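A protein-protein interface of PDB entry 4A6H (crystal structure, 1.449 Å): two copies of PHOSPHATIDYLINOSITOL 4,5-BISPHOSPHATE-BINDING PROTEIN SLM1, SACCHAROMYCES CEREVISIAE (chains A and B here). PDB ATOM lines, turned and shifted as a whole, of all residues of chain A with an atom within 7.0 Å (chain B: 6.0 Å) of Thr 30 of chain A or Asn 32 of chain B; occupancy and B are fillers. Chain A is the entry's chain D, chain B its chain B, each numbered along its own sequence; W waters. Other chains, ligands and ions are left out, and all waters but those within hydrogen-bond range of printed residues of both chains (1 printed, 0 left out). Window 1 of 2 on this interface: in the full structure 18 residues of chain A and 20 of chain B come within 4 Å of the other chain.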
ATOM      1  N   PRO A   3       0.899  -3.673 -18.044  1.00  0.00           N
ATOM      2  CA  PRO A   3       0.618  -4.407 -19.283  1.00  0.00           C
ATOM      3  C   PRO A   3       1.835  -4.464 -20.205  1.00  0.00           C
ATOM      4  O   PRO A   3       1.897  -3.692 -21.164  1.00  0.00           O
ATOM      5  CB  PRO A   3      -0.486  -3.571 -19.943  1.00  0.00           C
ATOM      6  CG  PRO A   3      -1.100  -2.796 -18.843  1.00  0.00           C
ATOM      7  CD  PRO A   3      -0.005  -2.525 -17.863  1.00  0.00           C
ATOM      8  N   PHE A   4       2.784  -5.354 -19.928  1.00  0.00           N
ATOM      9  CA  PHE A   4       3.954  -5.472 -20.795  1.00  0.00           C
ATOM     10  C   PHE A   4       3.643  -6.260 -22.061  1.00  0.00           C
ATOM     11  O   PHE A   4       2.592  -6.889 -22.180  1.00  0.00           O
ATOM     12  CB  PHE A   4       5.179  -6.060 -20.055  1.00  0.00           C
ATOM     13  N   THR A   5       4.569  -6.210 -23.008  1.00  0.00           N
ATOM     14  CA  THR A   5       4.579  -7.147 -24.110  1.00  0.00           C
ATOM     15  C   THR A   5       6.051  -7.421 -24.391  1.00  0.00           C
ATOM     16  O   THR A   5       6.691  -6.660 -25.118  1.00  0.00           O
ATOM     17  CB  THR A   5       3.921  -6.571 -25.378  1.00  0.00           C
ATOM     18  OG1 THR A   5       2.566  -6.194 -25.101  1.00  0.00           O
ATOM     19  CG2 THR A   5       3.938  -7.602 -26.502  1.00  0.00           C
ATOM     20  N   GLU A   6       6.601  -8.468 -23.778  1.00  0.00           N
ATOM     21  CA  GLU A   6       7.989  -8.857 -24.056  1.00  0.00           C
ATOM     22  C   GLU A   6       8.076 -10.319 -24.459  1.00  0.00           C
ATOM     23  O   GLU A   6       7.295 -11.157 -24.006  1.00  0.00           O
ATOM     24  CB  GLU A   6       8.899  -8.593 -22.860  1.00  0.00           C
ATOM     25  CG  GLU A   6       9.086  -9.805 -21.957  1.00  0.00           C
ATOM     26  CD  GLU A   6      10.094  -9.573 -20.848  1.00  0.00           C
ATOM     27  OE1 GLU A   6      10.436  -8.399 -20.575  1.00  0.00           O
ATOM     28  OE2 GLU A   6      10.536 -10.571 -20.243  1.00  0.00           O
ATOM     29  N   ILE A   7       9.047 -10.620 -25.310  1.00  0.00           N
ATOM     30  CA  ILE A   7       9.227 -11.957 -25.838  1.00  0.00           C
ATOM     31  C   ILE A   7      10.268 -12.690 -25.007  1.00  0.00           C
ATOM     32  O   ILE A   7      10.101 -13.854 -24.651  1.00  0.00           O
ATOM     33  CB  ILE A   7       9.679 -11.868 -27.295  1.00  0.00           C
ATOM     34  CG1 ILE A   7       8.545 -11.281 -28.143  1.00  0.00           C
ATOM     35  CG2 ILE A   7      10.095 -13.233 -27.825  1.00  0.00           C
ATOM     36  CD1 ILE A   7       8.934 -10.978 -29.559  1.00  0.00           C
ATOM     37  N   LYS A   8      11.344 -11.987 -24.684  1.00  0.00           N
ATOM     38  CA  LYS A   8      12.407 -12.569 -23.894  1.00  0.00           C
ATOM     39  C   LYS A   8      13.165 -11.470 -23.174  1.00  0.00           C
ATOM     40  O   LYS A   8      13.252 -10.352 -23.673  1.00  0.00           O
ATOM     41  CB  LYS A   8      13.360 -13.358 -24.796  1.00  0.00           C
ATOM     42  CG  LYS A   8      14.408 -14.133 -24.036  1.00  0.00           C
ATOM     43  CD  LYS A   8      15.072 -15.167 -24.913  1.00  0.00           C
ATOM     44  CE  LYS A   8      16.087 -15.981 -24.132  1.00  0.00           C
ATOM     45  NZ  LYS A   8      15.427 -16.977 -23.236  1.00  0.00           N
ATOM     46  N   VAL A  28      16.026  -6.714 -23.346  1.00  0.00           N
ATOM     47  CA  VAL A  28      14.615  -7.031 -23.449  1.00  0.00           C
ATOM     48  C   VAL A  28      14.238  -7.048 -24.913  1.00  0.00           C
ATOM     49  O   VAL A  28      14.411  -6.059 -25.634  1.00  0.00           O
ATOM     50  CB  VAL A  28      13.761  -6.007 -22.705  1.00  0.00           C
ATOM     51  CG1 VAL A  28      12.275  -6.351 -22.834  1.00  0.00           C
ATOM     52  CG2 VAL A  28      14.187  -5.963 -21.232  1.00  0.00           C
ATOM     53  N   LEU A  29      13.770  -8.204 -25.361  1.00  0.00           N
ATOM     54  CA  LEU A  29      13.328  -8.374 -26.735  1.00  0.00           C
ATOM     55  C   LEU A  29      11.821  -8.237 -26.799  1.00  0.00           C
ATOM     56  O   LEU A  29      11.100  -8.952 -26.096  1.00  0.00           O
ATOM     57  CB  LEU A  29      13.723  -9.761 -27.219  1.00  0.00           C
ATOM     58  CG  LEU A  29      13.351 -10.122 -28.651  1.00  0.00           C
ATOM     59  CD1 LEU A  29      14.051  -9.195 -29.636  1.00  0.00           C
ATOM     60  CD2 LEU A  29      13.690 -11.597 -28.897  1.00  0.00           C
ATOM     61  N   THR A  30      11.358  -7.318 -27.638  1.00  0.00           N
ATOM     62  CA  THR A  30       9.932  -7.110 -27.841  1.00  0.00           C
ATOM     63  C   THR A  30       9.659  -7.379 -29.318  1.00  0.00           C
ATOM     64  O   THR A  30      10.572  -7.635 -30.078  1.00  0.00           O
ATOM     65  CB  THR A  30       9.521  -5.669 -27.491  1.00  0.00           C
ATOM     66  OG1 THR A  30      10.060  -4.773 -28.465  1.00  0.00           O
ATOM     67  CG2 THR A  30       9.995  -5.267 -26.091  1.00  0.00           C
ATOM     68  N   PRO A  31       8.387  -7.328 -29.734  1.00  0.00           N
ATOM     69  CA  PRO A  31       8.168  -7.547 -31.163  1.00  0.00           C
ATOM     70  C   PRO A  31       8.860  -6.511 -32.039  1.00  0.00           C
ATOM     71  O   PRO A  31       9.067  -6.771 -33.216  1.00  0.00           O
ATOM     72  CB  PRO A  31       6.645  -7.437 -31.291  1.00  0.00           C
ATOM     73  CG  PRO A  31       6.140  -7.931 -29.967  1.00  0.00           C
ATOM     74  CD  PRO A  31       7.139  -7.394 -28.953  1.00  0.00           C
ATOM     75  N   ASN A  32       9.223  -5.361 -31.469  1.00  0.00           N
ATOM     76  CA  ASN A  32       9.766  -4.252 -32.256  1.00  0.00           C
ATOM     77  C   ASN A  32      11.261  -3.973 -32.094  1.00  0.00           C
ATOM     78  O   ASN A  32      11.909  -3.482 -33.012  1.00  0.00           O
ATOM     79  CB  ASN A  32       9.014  -2.957 -31.911  1.00  0.00           C
ATOM     80  CG  ASN A  32       7.502  -3.102 -32.003  1.00  0.00           C
ATOM     81  OD1 ASN A  32       6.984  -3.692 -32.943  1.00  0.00           O
ATOM     82  ND2 ASN A  32       6.795  -2.552 -31.025  1.00  0.00           N
ATOM     83  N   PHE A  33      11.789  -4.231 -30.902  1.00  0.00           N
ATOM     84  CA  PHE A  33      13.141  -3.805 -30.568  1.00  0.00           C
ATOM     85  C   PHE A  33      13.880  -4.858 -29.771  1.00  0.00           C
ATOM     86  O   PHE A  33      13.282  -5.653 -29.034  1.00  0.00           O
ATOM     87  CB  PHE A  33      13.097  -2.531 -29.686  1.00  0.00           C
ATOM     88  CG  PHE A  33      12.712  -1.273 -30.418  1.00  0.00           C
ATOM     89  CD1 PHE A  33      13.602  -0.643 -31.261  1.00  0.00           C
ATOM     90  CD2 PHE A  33      11.481  -0.696 -30.209  1.00  0.00           C
ATOM     91  CE1 PHE A  33      13.256   0.517 -31.918  1.00  0.00           C
ATOM     92  CE2 PHE A  33      11.133   0.462 -30.855  1.00  0.00           C
ATOM     93  CZ  PHE A  33      12.013   1.071 -31.711  1.00  0.00           C
ATOM     94  N   LEU A  34      15.196  -4.845 -29.909  1.00  0.00           N
ATOM     95  CA  LEU A  34      16.045  -5.378 -28.867  1.00  0.00           C
ATOM     96  C   LEU A  34      16.525  -4.175 -28.051  1.00  0.00           C
ATOM     97  O   LEU A  34      17.321  -3.358 -28.542  1.00  0.00           O
ATOM     98  CB  LEU A  34      17.203  -6.174 -29.474  1.00  0.00           C
ATOM     99  CG  LEU A  34      18.211  -6.738 -28.478  1.00  0.00           C
ATOM    100  CD1 LEU A  34      17.544  -7.757 -27.571  1.00  0.00           C
ATOM    101  CD2 LEU A  34      19.350  -7.380 -29.258  1.00  0.00           C
ATOM    102  N   HIS A  35      15.999  -4.050 -26.826  1.00  0.00           N
ATOM    103  CA  HIS A  35      16.405  -2.971 -25.925  1.00  0.00           C
ATOM    104  C   HIS A  35      17.526  -3.423 -24.997  1.00  0.00           C
ATOM    105  O   HIS A  35      17.490  -4.544 -24.486  1.00  0.00           O
ATOM    106  CB  HIS A  35      15.251  -2.540 -25.006  1.00  0.00           C
ATOM    107  CG  HIS A  35      14.037  -2.021 -25.714  1.00  0.00           C
ATOM    108  ND1 HIS A  35      14.027  -0.819 -26.385  1.00  0.00           N
ATOM    109  CD2 HIS A  35      12.776  -2.513 -25.801  1.00  0.00           C
ATOM    110  CE1 HIS A  35      12.815  -0.598 -26.868  1.00  0.00           C
ATOM    111  NE2 HIS A  35      12.043  -1.615 -26.541  1.00  0.00           N
ATOM    112  N   LEU A  54      14.268  -4.160 -34.828  1.00  0.00           N
ATOM    113  CA  LEU A  54      14.359  -5.479 -35.449  1.00  0.00           C
ATOM    114  C   LEU A  54      14.110  -5.479 -36.958  1.00  0.00           C
ATOM    115  O   LEU A  54      14.678  -6.299 -37.675  1.00  0.00           O
ATOM    116  CB  LEU A  54      13.404  -6.453 -34.767  1.00  0.00           C
ATOM    117  CG  LEU A  54      13.590  -6.642 -33.261  1.00  0.00           C
ATOM    118  CD1 LEU A  54      12.596  -7.657 -32.734  1.00  0.00           C
ATOM    119  CD2 LEU A  54      15.011  -7.083 -32.957  1.00  0.00           C
ATOM    120  N   LEU A 113      14.699 -14.240 -32.553  1.00  0.00           N
ATOM    121  CA  LEU A 113      15.214 -13.221 -33.454  1.00  0.00           C
ATOM    122  C   LEU A 113      15.083 -13.614 -34.920  1.00  0.00           C
ATOM    123  O   LEU A 113      14.798 -12.769 -35.767  1.00  0.00           O
ATOM    124  CB  LEU A 113      16.672 -12.918 -33.108  1.00  0.00           C
ATOM    125  CG  LEU A 113      16.816 -12.034 -31.865  1.00  0.00           C
ATOM    126  CD1 LEU A 113      18.247 -12.062 -31.347  1.00  0.00           C
ATOM    127  CD2 LEU A 113      16.361 -10.602 -32.132  1.00  0.00           C
ATOM    128  N   LEU A 116      11.463 -13.032 -35.882  1.00  0.00           N
ATOM    129  CA  LEU A 116      11.158 -11.606 -35.857  1.00  0.00           C
ATOM    130  C   LEU A 116      11.789 -10.838 -37.011  1.00  0.00           C
ATOM    131  O   LEU A 116      11.221  -9.859 -37.488  1.00  0.00           O
ATOM    132  CB  LEU A 116      11.586 -10.989 -34.523  1.00  0.00           C
ATOM    133  CG  LEU A 116      10.860 -11.586 -33.318  1.00  0.00           C
ATOM    134  CD1 LEU A 116      11.510 -11.180 -32.005  1.00  0.00           C
ATOM    135  CD2 LEU A 116       9.396 -11.142 -33.338  1.00  0.00           C
ATOM    136  N   THR B  30       3.193   2.035 -28.108  1.00  0.00           N
ATOM    137  CA  THR B  30       3.146   0.567 -28.047  1.00  0.00           C
ATOM    138  C   THR B  30       2.623   0.162 -26.665  1.00  0.00           C
ATOM    139  O   THR B  30       2.421   1.006 -25.809  1.00  0.00           O
ATOM    140  CB  THR B  30       4.541  -0.059 -28.242  1.00  0.00           C
ATOM    141  OG1 THR B  30       5.337   0.182 -27.075  1.00  0.00           O
ATOM    142  CG2 THR B  30       5.225   0.514 -29.463  1.00  0.00           C
ATOM    143  N   PRO B  31       2.425  -1.141 -26.428  1.00  0.00           N
ATOM    144  CA  PRO B  31       2.019  -1.479 -25.061  1.00  0.00           C
ATOM    145  C   PRO B  31       3.063  -1.141 -23.982  1.00  0.00           C
ATOM    146  O   PRO B  31       2.703  -1.114 -22.801  1.00  0.00           O
ATOM    147  CB  PRO B  31       1.791  -2.996 -25.134  1.00  0.00           C
ATOM    148  CG  PRO B  31       1.438  -3.245 -26.549  1.00  0.00           C
ATOM    149  CD  PRO B  31       2.296  -2.287 -27.341  1.00  0.00           C
ATOM    150  N   ASN B  32       4.313  -0.878 -24.368  1.00  0.00           N
ATOM    151  CA  ASN B  32       5.383  -0.640 -23.399  1.00  0.00           C
ATOM    152  C   ASN B  32       5.843   0.806 -23.293  1.00  0.00           C
ATOM    153  O   ASN B  32       6.240   1.259 -22.225  1.00  0.00           O
ATOM    154  CB  ASN B  32       6.593  -1.522 -23.722  1.00  0.00           C
ATOM    155  CG  ASN B  32       6.260  -2.988 -23.697  1.00  0.00           C
ATOM    156  OD1 ASN B  32       5.636  -3.473 -22.754  1.00  0.00           O
ATOM    157  ND2 ASN B  32       6.668  -3.707 -24.734  1.00  0.00           N
ATOM    158  N   PHE B  33       5.807   1.529 -24.409  1.00  0.00           N
ATOM    159  CA  PHE B  33       6.425   2.843 -24.484  1.00  0.00           C
ATOM    160  C   PHE B  33       5.597   3.803 -25.310  1.00  0.00           C
ATOM    161  O   PHE B  33       4.850   3.390 -26.206  1.00  0.00           O
ATOM    162  CB  PHE B  33       7.798   2.758 -25.180  1.00  0.00           C
ATOM    163  CG  PHE B  33       8.877   2.103 -24.360  1.00  0.00           C
ATOM    164  CD1 PHE B  33       9.534   2.805 -23.351  1.00  0.00           C
ATOM    165  CD2 PHE B  33       9.266   0.809 -24.630  1.00  0.00           C
ATOM    166  CE1 PHE B  33      10.542   2.203 -22.606  1.00  0.00           C
ATOM    167  CE2 PHE B  33      10.269   0.198 -23.885  1.00  0.00           C
ATOM    168  CZ  PHE B  33      10.904   0.902 -22.874  1.00  0.00           C
ATOM    169  N   LEU B  34       5.729   5.088 -24.985  1.00  0.00           N
ATOM    170  CA  LEU B  34       5.456   6.138 -25.942  1.00  0.00           C
ATOM    171  C   LEU B  34       6.817   6.546 -26.519  1.00  0.00           C
ATOM    172  O   LEU B  34       7.669   7.106 -25.801  1.00  0.00           O
ATOM    173  CB  LEU B  34       4.741   7.313 -25.255  1.00  0.00           C
ATOM    174  CG  LEU B  34       4.449   8.481 -26.198  1.00  0.00           C
ATOM    175  CD1 LEU B  34       3.438   8.070 -27.256  1.00  0.00           C
ATOM    176  CD2 LEU B  34       3.946   9.679 -25.409  1.00  0.00           C
ATOM    177  N   LEU B  52       9.421   6.665 -23.561  1.00  0.00           N
ATOM    178  CA  LEU B  52       8.843   6.898 -22.248  1.00  0.00           C
ATOM    179  C   LEU B  52       8.117   5.658 -21.779  1.00  0.00           C
ATOM    180  O   LEU B  52       7.099   5.275 -22.361  1.00  0.00           O
ATOM    181  CB  LEU B  52       7.816   8.029 -22.325  1.00  0.00           C
ATOM    182  CG  LEU B  52       8.345   9.421 -22.631  1.00  0.00           C
ATOM    183  CD1 LEU B  52       7.235  10.308 -23.190  1.00  0.00           C
ATOM    184  CD2 LEU B  52       8.941  10.038 -21.382  1.00  0.00           C
ATOM    185  N   ALA B  53       8.618   5.046 -20.707  1.00  0.00           N
ATOM    186  CA  ALA B  53       8.044   3.807 -20.194  1.00  0.00           C
ATOM    187  C   ALA B  53       6.667   4.042 -19.596  1.00  0.00           C
ATOM    188  O   ALA B  53       6.526   4.813 -18.651  1.00  0.00           O
ATOM    189  CB  ALA B  53       8.967   3.202 -19.160  1.00  0.00           C
ATOM    190  N   LEU B  54       5.666   3.356 -20.133  1.00  0.00           N
ATOM    191  CA  LEU B  54       4.289   3.574 -19.724  1.00  0.00           C
ATOM    192  C   LEU B  54       4.067   3.076 -18.292  1.00  0.00           C
ATOM    193  O   LEU B  54       3.179   3.556 -17.607  1.00  0.00           O
ATOM    194  CB  LEU B  54       3.333   2.876 -20.690  1.00  0.00           C
ATOM    195  CG  LEU B  54       3.387   3.378 -22.132  1.00  0.00           C
ATOM    196  CD1 LEU B  54       2.402   2.594 -22.989  1.00  0.00           C
ATOM    197  CD2 LEU B  54       3.114   4.865 -22.166  1.00  0.00           C
ATOM    198  N   SER B  55       4.892   2.129 -17.854  1.00  0.00           N
ATOM    199  CA  SER B  55       4.761   1.548 -16.515  1.00  0.00           C
ATOM    200  C   SER B  55       4.915   2.596 -15.425  1.00  0.00           C
ATOM    201  O   SER B  55       4.436   2.418 -14.306  1.00  0.00           O
ATOM    202  CB  SER B  55       5.801   0.440 -16.304  1.00  0.00           C
ATOM    203  OG  SER B  55       7.122   0.946 -16.365  1.00  0.00           O
HETATM  204  O   HOH W   1       5.460  -5.007 -27.585  1.00  0.00           O
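N of Thr 5 of chain A sits at hydrogen-bond distance from OD1 of Asn 32 of chain B, at 2.9 Å.
O of Pro 31 of chain B sits close to O of Pro 3 of chain A.
The side-chain hydroxyl of Thr 30 of chain B lies close to the backbone NH of Asn 32 of chain B (3.1 Å).
OG1 of Thr 30 of chain B is in hydrogen-bond range of N of Phe 33 of chain B (3.0 Å).
N of Leu 54 of chain B sits at hydrogen-bond distance from O of Asn 32 of chain B (3.0 Å).
O of Val 28 of chain A is in hydrogen-bond range of N of His 35 of chain A (2.8 Å).
The side-chain hydroxyl (OG1) of Thr 30 of chain A lies close to the backbone NH (N) of Asn 32 of chain A (3.2 Å).
O of Asn 32 of chain A sits at hydrogen-bond distance from N of Leu 54 of chain A (3.1 Å).
Among the printed residues, merely in contact across the chains: Phe 4 of chain A with Asn 32 of chain B, Thr 5 of chain A with Pro 31 of chain B, His 35 of chain A with Phe 33 of chain B, Asn 32 of chain A with Thr 30 of chain B and Thr 30 of chain A with Asn 32 of chain B.
Printed residues of chain B within 4 Å of Pro 3 of chain A: Pro 31 (3.2 Å).
Thr 30 of chain A touches just one residue of chain B: Asn 32 (3.9 Å).
Phe 33 of chain A touches none of the printed residues of chain B.
Of the printed residues of chain A, Thr 30 of chain B touches Asn 32.
Of chain A, only Phe 4, Thr 5 and Thr 30 come within 4 Å of Asn 32 of chain B.
Of the printed residues of chain A, Phe 33 of chain B touches His 35 (3.7 Å).
The nearest residue of chain A that does not touch Asn 32 of chain B is Pro 3 of chain A (4.1 Å).
The nearest printed residue of chain A that does not touch Pro 31 of chain B is Phe 4 of chain A (4.9 Å).
Among the printed residues, 7 pairs touch across the chains.
Among the printed residues, no Asp or Glu carboxylate lies within 4 Å of a Lys or Arg side-chain nitrogen of the other chain.
Thr 30 of chain A touches Asn 32 of chain B, and with the chains exchanged Asn 32 of chain A touches Thr 30 of chain B.
Positions printed for both chains: 30, 31, 32, 33, 34 and 54.
Of the 7 pairs that touch across the chains among the printed residues, 2 have their exchanged pair printed and touching as well.
Water W1 lies within hydrogen-bond range of the backbone carbonyl oxygen of Thr 5 of chain A (3.2 Å) and the side-chain amide nitrogen of Asn 32 of chain B (3.4 Å).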
